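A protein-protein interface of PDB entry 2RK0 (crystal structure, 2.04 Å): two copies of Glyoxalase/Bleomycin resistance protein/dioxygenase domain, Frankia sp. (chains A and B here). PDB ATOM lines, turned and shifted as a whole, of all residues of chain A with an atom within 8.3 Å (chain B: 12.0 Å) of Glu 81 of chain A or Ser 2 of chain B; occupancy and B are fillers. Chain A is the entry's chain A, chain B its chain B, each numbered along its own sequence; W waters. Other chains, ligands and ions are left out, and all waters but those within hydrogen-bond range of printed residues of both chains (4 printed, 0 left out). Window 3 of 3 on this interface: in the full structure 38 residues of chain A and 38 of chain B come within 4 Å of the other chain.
Water W2 lies within hydrogen-bond range of OG of Ser 82 of chain A (2.4 Å), OD2 of Asp 85 of chain A (3.2 Å) and N of Ser 2 of chain B (3.4 Å). Water W1 lies within hydrogen-bond range of the backbone carbonyl oxygen (O) of Ser 4 of chain B (2.7 Å), the backbone carbonyl oxygen (O) of Pro 48 of chain A (2.8 Å) and the backbone NH (N) of Gly 50 of chain A (3.3 Å). Water W3 lies within hydrogen-bond range of OG of Ser 79 of chain A (2.8 Å) and O of Val 6 of chain B (3.3 Å). Water W4 bridges OG of Ser 4 of chain B and O of Val 80 of chain A.
No position is printed for both chains.
Of chain A, only Val 80, Glu 81 and Asp 85 come within 4 Å of Ser 2 of chain B. Gly 49 of chain A touches just these residues of chain B: Leu 3 and Ser 4. Ser 79 of chain A touches just these residues of chain B: Leu 3, Ser 4, Gly 5, Val 6 and Ser 7. Of chain B, only Ser 2 comes within 4 Å of Val 80 of chain A. No residue of chain B comes within 4 Å of Ser 82 of chain A. Of chain B, only Ser 2 (2.9 Å) comes within 4 Å of Asp 85 of chain A. No residue of chain B comes within 4 Å of Gly 127 of chain A. Of the printed residues of chain A, Ser 7 of chain B touches Phe 78, Ser 79 and Met 125. Printed residues of chain B within 4 Å of Met 125 of chain A: Ser 7. Of the printed residues of chain A, Ser 4 of chain B touches Gly 49 and Ser 79. Of the printed residues of chain B, Phe 78 of chain A touches Leu 3 (3.8 Å), Gly 5 (3.3 Å) and Ser 7 (3.9 Å). Printed residues of chain A within 4 Å of Val 6 of chain B: Ser 79 (3.9 Å). Leu 47 of chain A touches none of the printed residues of chain B. His 132 of chain A touches none of the printed residues of chain B. The nearest printed residue of chain A that does not touch Val 6 of chain B is Phe 78 of chain A (4.4 Å).
Hydrophobic or aromatic side chains of chain B that line the printed part of chain A: Leu 3. Hydrophobic or aromatic side chains of chain A that line the printed part of chain B: Phe 78 and Met 125. Among the printed residues, 15 pairs touch across the chains.
Among the printed residues, merely in contact across the chains: Phe 78 of chain A with Gly 5 of chain B, Gly 49 of chain A with Leu 3 of chain B, Ser 79 of chain A with Leu 3 of chain B, Val 80 of chain A with Ser 2 of chain B, Phe 78 of chain A with Leu 3 of chain B, Met 125 of chain A with Ser 7 of chain B, Ser 79 of chain A with Val 6 of chain B and Phe 78 of chain A with Ser 7 of chain B.
The backbone carbonyl oxygen of Ser 79 of chain A lies within hydrogen-bond range of the backbone NH of Ser 4 of chain B, 2.9 Å away. O of Gly 5 of chain B sits at hydrogen-bond distance from N of Ser 79 of chain A (2.8 Å). The side-chain hydroxyl (OG) of Ser 79 of chain A lies close to the backbone NH (N) of Ser 7 of chain B, at 3.5 Å. The side-chain carboxylate (OE1) of Glu 81 of chain A lies within hydrogen-bond range of the backbone NH (N) of Ser 2 of chain B. The side-chain carboxylate (OD2) of Asp 85 of chain A lies within hydrogen-bond range of the backbone NH (N) of Ser 2 of chain B, 2.9 Å away. O of Leu 3 of chain B lies close to O of Pro 48 of chain A (2.9 Å). O of Gly 49 of chain A sits close to O of Ser 4 of chain B (3.0 Å).
O of Phe 78 of chain A is in hydrogen-bond range of N of Met 125 of chain A (2.8 Å). N of Val 80 of chain A lies within hydrogen-bond range of O of Met 125 of chain A (2.9 Å). OD2 of Asp 85 of chain A is in hydrogen-bond range of N of Glu 81 of chain A, at 3.1 Å. OD2 of Asp 85 of chain A is in hydrogen-bond range of N of Ser 82 of chain A (3.0 Å).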
ATOM      1  N   LEU A  27     -21.601 -28.506  15.527  1.00  0.00           N
ATOM      2  CA  LEU A  27     -20.336 -28.916  16.129  1.00  0.00           C
ATOM      3  C   LEU A  27     -19.120 -28.817  15.220  1.00  0.00           C
ATOM      4  O   LEU A  27     -18.049 -29.312  15.569  1.00  0.00           O
ATOM      5  CB  LEU A  27     -20.463 -30.351  16.650  1.00  0.00           C
ATOM      6  CG  LEU A  27     -21.634 -30.625  17.595  1.00  0.00           C
ATOM      7  CD1 LEU A  27     -21.752 -32.124  17.847  1.00  0.00           C
ATOM      8  CD2 LEU A  27     -21.438 -29.870  18.900  1.00  0.00           C
ATOM      9  N   ASP A  28     -19.274 -28.174  14.069  1.00  0.00           N
ATOM     10  CA  ASP A  28     -18.162 -28.046  13.132  1.00  0.00           C
ATOM     11  C   ASP A  28     -17.660 -29.411  12.718  1.00  0.00           C
ATOM     12  O   ASP A  28     -16.476 -29.596  12.440  1.00  0.00           O
ATOM     13  CB  ASP A  28     -17.006 -27.253  13.742  1.00  0.00           C
ATOM     14  CG  ASP A  28     -17.350 -25.798  13.939  1.00  0.00           C
ATOM     15  OD1 ASP A  28     -17.895 -25.202  12.989  1.00  0.00           O
ATOM     16  OD2 ASP A  28     -17.073 -25.264  15.033  1.00  0.00           O
ATOM     17  N   LEU A  47     -14.743 -34.186  14.431  1.00  0.00           N
ATOM     18  CA  LEU A  47     -15.053 -32.954  15.145  1.00  0.00           C
ATOM     19  C   LEU A  47     -13.769 -32.252  15.543  1.00  0.00           C
ATOM     20  O   LEU A  47     -12.695 -32.851  15.540  1.00  0.00           O
ATOM     21  CB  LEU A  47     -15.814 -33.257  16.438  1.00  0.00           C
ATOM     22  CG  LEU A  47     -17.121 -34.043  16.411  1.00  0.00           C
ATOM     23  CD1 LEU A  47     -17.540 -34.299  17.839  1.00  0.00           C
ATOM     24  CD2 LEU A  47     -18.196 -33.278  15.665  1.00  0.00           C
ATOM     25  N   PRO A  48     -13.858 -30.956  15.862  1.00  0.00           N
ATOM     26  CA  PRO A  48     -12.633 -30.275  16.275  1.00  0.00           C
ATOM     27  C   PRO A  48     -12.192 -31.063  17.515  1.00  0.00           C
ATOM     28  O   PRO A  48     -13.039 -31.532  18.285  1.00  0.00           O
ATOM     29  CB  PRO A  48     -13.125 -28.879  16.623  1.00  0.00           C
ATOM     30  CG  PRO A  48     -14.238 -28.671  15.614  1.00  0.00           C
ATOM     31  CD  PRO A  48     -14.961 -30.000  15.644  1.00  0.00           C
ATOM     32  N   GLY A  49     -10.889 -31.229  17.703  1.00  0.00           N
ATOM     33  CA  GLY A  49     -10.419 -31.984  18.845  1.00  0.00           C
ATOM     34  C   GLY A  49     -10.065 -33.401  18.440  1.00  0.00           C
ATOM     35  O   GLY A  49      -9.378 -34.105  19.175  1.00  0.00           O
ATOM     36  N   GLY A  50     -10.554 -33.835  17.279  1.00  0.00           N
ATOM     37  CA  GLY A  50     -10.224 -35.168  16.792  1.00  0.00           C
ATOM     38  C   GLY A  50     -11.240 -36.302  16.855  1.00  0.00           C
ATOM     39  O   GLY A  50     -11.037 -37.331  16.205  1.00  0.00           O
ATOM     40  N   PHE A  78     -19.481 -34.358  25.496  1.00  0.00           N
ATOM     41  CA  PHE A  78     -18.220 -33.868  24.944  1.00  0.00           C
ATOM     42  C   PHE A  78     -17.506 -32.934  25.923  1.00  0.00           C
ATOM     43  O   PHE A  78     -18.148 -32.213  26.687  1.00  0.00           O
ATOM     44  CB  PHE A  78     -18.477 -33.086  23.647  1.00  0.00           C
ATOM     45  CG  PHE A  78     -19.267 -33.844  22.609  1.00  0.00           C
ATOM     46  CD1 PHE A  78     -18.720 -34.951  21.964  1.00  0.00           C
ATOM     47  CD2 PHE A  78     -20.552 -33.433  22.259  1.00  0.00           C
ATOM     48  CE1 PHE A  78     -19.440 -35.638  20.983  1.00  0.00           C
ATOM     49  CE2 PHE A  78     -21.281 -34.114  21.279  1.00  0.00           C
ATOM     50  CZ  PHE A  78     -20.721 -35.217  20.641  1.00  0.00           C
ATOM     51  N   SER A  79     -16.177 -32.943  25.889  1.00  0.00           N
ATOM     52  CA  SER A  79     -15.396 -32.049  26.737  1.00  0.00           C
ATOM     53  C   SER A  79     -15.113 -30.785  25.928  1.00  0.00           C
ATOM     54  O   SER A  79     -14.776 -30.880  24.748  1.00  0.00           O
ATOM     55  CB  SER A  79     -14.050 -32.684  27.121  1.00  0.00           C
ATOM     56  OG  SER A  79     -14.207 -33.783  27.996  1.00  0.00           O
ATOM     57  N   VAL A  80     -15.275 -29.615  26.544  1.00  0.00           N
ATOM     58  CA  VAL A  80     -14.960 -28.350  25.881  1.00  0.00           C
ATOM     59  C   VAL A  80     -13.896 -27.663  26.736  1.00  0.00           C
ATOM     60  O   VAL A  80     -13.783 -27.933  27.934  1.00  0.00           O
ATOM     61  CB  VAL A  80     -16.200 -27.425  25.719  1.00  0.00           C
ATOM     62  CG1 VAL A  80     -17.217 -28.092  24.798  1.00  0.00           C
ATOM     63  CG2 VAL A  80     -16.812 -27.104  27.079  1.00  0.00           C
ATOM     64  N   GLU A  81     -13.123 -26.774  26.132  1.00  0.00           N
ATOM     65  CA  GLU A  81     -12.034 -26.107  26.837  1.00  0.00           C
ATOM     66  C   GLU A  81     -12.336 -24.837  27.618  1.00  0.00           C
ATOM     67  O   GLU A  81     -11.704 -24.585  28.646  1.00  0.00           O
ATOM     68  CB  GLU A  81     -10.905 -25.838  25.843  1.00  0.00           C
ATOM     69  CG  GLU A  81     -10.433 -27.105  25.150  1.00  0.00           C
ATOM     70  CD  GLU A  81      -9.405 -26.842  24.074  1.00  0.00           C
ATOM     71  OE1 GLU A  81      -9.595 -25.888  23.285  1.00  0.00           O
ATOM     72  OE2 GLU A  81      -8.413 -27.596  24.011  1.00  0.00           O
ATOM     73  N   SER A  82     -13.286 -24.034  27.153  1.00  0.00           N
ATOM     74  CA  SER A  82     -13.603 -22.801  27.868  1.00  0.00           C
ATOM     75  C   SER A  82     -15.086 -22.489  27.820  1.00  0.00           C
ATOM     76  O   SER A  82     -15.831 -23.127  27.090  1.00  0.00           O
ATOM     77  CB  SER A  82     -12.838 -21.631  27.254  1.00  0.00           C
ATOM     78  OG  SER A  82     -13.330 -21.370  25.956  1.00  0.00           O
ATOM     79  N   MET A  83     -15.496 -21.500  28.606  1.00  0.00           N
ATOM     80  CA  MET A  83     -16.882 -21.068  28.659  1.00  0.00           C
ATOM     81  C   MET A  83     -17.324 -20.564  27.282  1.00  0.00           C
ATOM     82  O   MET A  83     -18.468 -20.757  26.881  1.00  0.00           O
ATOM     83  CB  MET A  83     -17.045 -19.942  29.683  1.00  0.00           C
ATOM     84  CG  MET A  83     -18.486 -19.544  29.942  1.00  0.00           C
ATOM     85  SD  MET A  83     -19.380 -20.932  30.942  1.00  0.00           S
ATOM     86  CE  MET A  83     -18.490 -20.774  32.658  1.00  0.00           C
ATOM     87  N   THR A  84     -16.408 -19.920  26.562  1.00  0.00           N
ATOM     88  CA  THR A  84     -16.717 -19.393  25.238  1.00  0.00           C
ATOM     89  C   THR A  84     -17.222 -20.499  24.322  1.00  0.00           C
ATOM     90  O   THR A  84     -18.106 -20.270  23.500  1.00  0.00           O
ATOM     91  CB  THR A  84     -15.489 -18.712  24.608  1.00  0.00           C
ATOM     92  OG1 THR A  84     -15.172 -17.529  25.356  1.00  0.00           O
ATOM     93  CG2 THR A  84     -15.774 -18.328  23.168  1.00  0.00           C
ATOM     94  N   ASP A  85     -16.669 -21.699  24.464  1.00  0.00           N
ATOM     95  CA  ASP A  85     -17.118 -22.818  23.654  1.00  0.00           C
ATOM     96  C   ASP A  85     -18.611 -23.059  23.906  1.00  0.00           C
ATOM     97  O   ASP A  85     -19.376 -23.308  22.974  1.00  0.00           O
ATOM     98  CB  ASP A  85     -16.328 -24.085  23.994  1.00  0.00           C
ATOM     99  CG  ASP A  85     -14.893 -24.020  23.513  1.00  0.00           C
ATOM    100  OD1 ASP A  85     -14.677 -23.555  22.372  1.00  0.00           O
ATOM    101  OD2 ASP A  85     -13.991 -24.448  24.267  1.00  0.00           O
ATOM    102  N   LEU A  86     -19.016 -22.987  25.167  1.00  0.00           N
ATOM    103  CA  LEU A  86     -20.417 -23.192  25.534  1.00  0.00           C
ATOM    104  C   LEU A  86     -21.276 -22.042  25.031  1.00  0.00           C
ATOM    105  O   LEU A  86     -22.394 -22.253  24.558  1.00  0.00           O
ATOM    106  CB  LEU A  86     -20.552 -23.315  27.061  1.00  0.00           C
ATOM    107  CG  LEU A  86     -19.876 -24.557  27.663  1.00  0.00           C
ATOM    108  CD1 LEU A  86     -20.177 -24.657  29.150  1.00  0.00           C
ATOM    109  CD2 LEU A  86     -20.368 -25.809  26.942  1.00  0.00           C
ATOM    110  N   LEU A  89     -21.849 -22.547  21.378  1.00  0.00           N
ATOM    111  CA  LEU A  89     -22.793 -23.637  21.141  1.00  0.00           C
ATOM    112  C   LEU A  89     -24.228 -23.156  21.361  1.00  0.00           C
ATOM    113  O   LEU A  89     -25.113 -23.425  20.553  1.00  0.00           O
ATOM    114  CB  LEU A  89     -22.515 -24.812  22.083  1.00  0.00           C
ATOM    115  CG  LEU A  89     -21.545 -25.896  21.623  1.00  0.00           C
ATOM    116  CD1 LEU A  89     -21.251 -26.854  22.771  1.00  0.00           C
ATOM    117  CD2 LEU A  89     -22.150 -26.640  20.441  1.00  0.00           C
ATOM    118  N   ALA A 124     -22.283 -30.866  26.507  1.00  0.00           N
ATOM    119  CA  ALA A 124     -20.980 -30.214  26.377  1.00  0.00           C
ATOM    120  C   ALA A 124     -20.638 -29.902  27.826  1.00  0.00           C
ATOM    121  O   ALA A 124     -21.444 -29.308  28.547  1.00  0.00           O
ATOM    122  CB  ALA A 124     -21.082 -28.946  25.580  1.00  0.00           C
ATOM    123  N   MET A 125     -19.439 -30.290  28.235  1.00  0.00           N
ATOM    124  CA  MET A 125     -19.002 -30.139  29.612  1.00  0.00           C
ATOM    125  C   MET A 125     -17.703 -29.356  29.822  1.00  0.00           C
ATOM    126  O   MET A 125     -16.727 -29.566  29.108  1.00  0.00           O
ATOM    127  CB  MET A 125     -18.846 -31.545  30.185  1.00  0.00           C
ATOM    128  CG  MET A 125     -17.959 -31.665  31.398  1.00  0.00           C
ATOM    129  SD  MET A 125     -19.035 -31.656  33.015  1.00  0.00           S
ATOM    130  CE  MET A 125     -18.684 -29.882  33.750  1.00  0.00           C
ATOM    131  N   LEU A 126     -17.704 -28.473  30.821  1.00  0.00           N
ATOM    132  CA  LEU A 126     -16.535 -27.664  31.177  1.00  0.00           C
ATOM    133  C   LEU A 126     -16.224 -27.912  32.652  1.00  0.00           C
ATOM    134  O   LEU A 126     -17.094 -27.751  33.511  1.00  0.00           O
ATOM    135  CB  LEU A 126     -16.814 -26.178  30.964  1.00  0.00           C
ATOM    136  CG  LEU A 126     -15.677 -25.210  31.330  1.00  0.00           C
ATOM    137  CD1 LEU A 126     -14.518 -25.376  30.340  1.00  0.00           C
ATOM    138  CD2 LEU A 126     -16.200 -23.765  31.312  1.00  0.00           C
ATOM    139  N   GLY A 127     -14.988 -28.301  32.945  1.00  0.00           N
ATOM    140  CA  GLY A 127     -14.602 -28.583  34.317  1.00  0.00           C
ATOM    141  C   GLY A 127     -14.369 -27.351  35.171  1.00  0.00           C
ATOM    142  O   GLY A 127     -14.096 -26.276  34.660  1.00  0.00           O
ATOM    143  N   HIS A 131      -9.242 -25.294  37.459  1.00  0.00           N
ATOM    144  CA  HIS A 131      -9.338 -24.290  36.408  1.00  0.00           C
ATOM    145  C   HIS A 131      -9.739 -22.962  37.049  1.00  0.00           C
ATOM    146  O   HIS A 131      -9.948 -22.893  38.260  1.00  0.00           O
ATOM    147  CB  HIS A 131     -10.393 -24.689  35.371  1.00  0.00           C
ATOM    148  CG  HIS A 131     -10.128 -26.008  34.711  1.00  0.00           C
ATOM    149  ND1 HIS A 131      -9.045 -26.225  33.893  1.00  0.00           N
ATOM    150  CD2 HIS A 131     -10.799 -27.183  34.776  1.00  0.00           C
ATOM    151  CE1 HIS A 131      -9.054 -27.485  33.482  1.00  0.00           C
ATOM    152  NE2 HIS A 131     -10.106 -28.085  34.004  1.00  0.00           N
ATOM    153  N   HIS A 132      -9.862 -21.917  36.236  1.00  0.00           N
ATOM    154  CA  HIS A 132     -10.236 -20.598  36.749  1.00  0.00           C
ATOM    155  C   HIS A 132     -11.418 -20.003  35.983  1.00  0.00           C
ATOM    156  O   HIS A 132     -11.586 -18.779  35.923  1.00  0.00           O
ATOM    157  CB  HIS A 132      -9.026 -19.664  36.659  1.00  0.00           C
ATOM    158  CG  HIS A 132      -7.874 -20.100  37.512  1.00  0.00           C
ATOM    159  ND1 HIS A 132      -7.926 -20.101  38.888  1.00  0.00           N
ATOM    160  CD2 HIS A 132      -6.651 -20.584  37.182  1.00  0.00           C
ATOM    161  CE1 HIS A 132      -6.787 -20.569  39.373  1.00  0.00           C
ATOM    162  NE2 HIS A 132      -5.998 -20.869  38.358  1.00  0.00           N
ATOM    163  N   HIS A 133     -12.234 -20.873  35.400  1.00  0.00           N
ATOM    164  CA  HIS A 133     -13.381 -20.431  34.621  1.00  0.00           C
ATOM    165  C   HIS A 133     -14.408 -19.695  35.468  1.00  0.00           C
ATOM    166  O   HIS A 133     -15.209 -18.927  34.938  1.00  0.00           O
ATOM    167  CB  HIS A 133     -14.047 -21.629  33.943  1.00  0.00           C
ATOM    168  CG  HIS A 133     -13.101 -22.471  33.144  1.00  0.00           C
ATOM    169  ND1 HIS A 133     -12.353 -21.969  32.104  1.00  0.00           N
ATOM    170  CD2 HIS A 133     -12.780 -23.785  33.241  1.00  0.00           C
ATOM    171  CE1 HIS A 133     -11.607 -22.937  31.592  1.00  0.00           C
ATOM    172  NE2 HIS A 133     -11.849 -24.047  32.265  1.00  0.00           N
ATOM    173  N   SER B   2     -11.836 -24.936  22.343  1.00  0.00           N
ATOM    174  CA  SER B   2     -12.851 -25.608  21.488  1.00  0.00           C
ATOM    175  C   SER B   2     -13.221 -26.955  22.092  1.00  0.00           C
ATOM    176  O   SER B   2     -12.891 -27.243  23.241  1.00  0.00           O
ATOM    177  CB  SER B   2     -12.300 -25.825  20.074  1.00  0.00           C
ATOM    178  OG  SER B   2     -11.323 -26.849  20.058  1.00  0.00           O
ATOM    179  N   LEU B   3     -13.913 -27.771  21.304  1.00  0.00           N
ATOM    180  CA  LEU B   3     -14.316 -29.095  21.745  1.00  0.00           C
ATOM    181  C   LEU B   3     -13.072 -29.965  21.632  1.00  0.00           C
ATOM    182  O   LEU B   3     -12.403 -29.966  20.602  1.00  0.00           O
ATOM    183  CB  LEU B   3     -15.436 -29.617  20.839  1.00  0.00           C
ATOM    184  CG  LEU B   3     -16.377 -30.693  21.387  1.00  0.00           C
ATOM    185  CD1 LEU B   3     -17.716 -30.572  20.686  1.00  0.00           C
ATOM    186  CD2 LEU B   3     -15.785 -32.089  21.200  1.00  0.00           C
ATOM    187  N   SER B   4     -12.747 -30.699  22.689  1.00  0.00           N
ATOM    188  CA  SER B   4     -11.560 -31.544  22.658  1.00  0.00           C
ATOM    189  C   SER B   4     -11.861 -33.008  22.353  1.00  0.00           C
ATOM    190  O   SER B   4     -11.294 -33.584  21.421  1.00  0.00           O
ATOM    191  CB  SER B   4     -10.798 -31.414  23.976  1.00  0.00           C
ATOM    192  OG  SER B   4     -11.679 -31.365  25.082  1.00  0.00           O
ATOM    193  N   GLY B   5     -12.750 -33.611  23.129  1.00  0.00           N
ATOM    194  CA  GLY B   5     -13.090 -35.001  22.897  1.00  0.00           C
ATOM    195  C   GLY B   5     -14.295 -35.456  23.698  1.00  0.00           C
ATOM    196  O   GLY B   5     -15.218 -34.681  23.937  1.00  0.00           O
ATOM    197  N   VAL B   6     -14.280 -36.717  24.116  1.00  0.00           N
ATOM    198  CA  VAL B   6     -15.375 -37.287  24.892  1.00  0.00           C
ATOM    199  C   VAL B   6     -15.156 -37.194  26.399  1.00  0.00           C
ATOM    200  O   VAL B   6     -14.170 -37.706  26.923  1.00  0.00           O
ATOM    201  CB  VAL B   6     -15.592 -38.771  24.532  1.00  0.00           C
ATOM    202  CG1 VAL B   6     -16.665 -39.375  25.428  1.00  0.00           C
ATOM    203  CG2 VAL B   6     -15.977 -38.894  23.066  1.00  0.00           C
ATOM    204  N   SER B   7     -16.083 -36.532  27.087  1.00  0.00           N
ATOM    205  CA  SER B   7     -16.030 -36.396  28.536  1.00  0.00           C
ATOM    206  C   SER B   7     -16.452 -37.749  29.125  1.00  0.00           C
ATOM    207  O   SER B   7     -15.827 -38.275  30.048  1.00  0.00           O
ATOM    208  CB  SER B   7     -16.995 -35.303  28.986  1.00  0.00           C
ATOM    209  OG  SER B   7     -17.003 -35.194  30.389  1.00  0.00           O
HETATM  210  O   HOH W   1     -13.005 -34.088  19.408  1.00  0.00           O
HETATM  211  O   HOH W   2     -11.793 -22.123  24.211  1.00  0.00           O
HETATM  212  O   HOH W   3     -11.989 -35.343  27.536  1.00  0.00           O
HETATM  213  O   HOH W   4     -11.105 -30.024  27.846  1.00  0.00           O
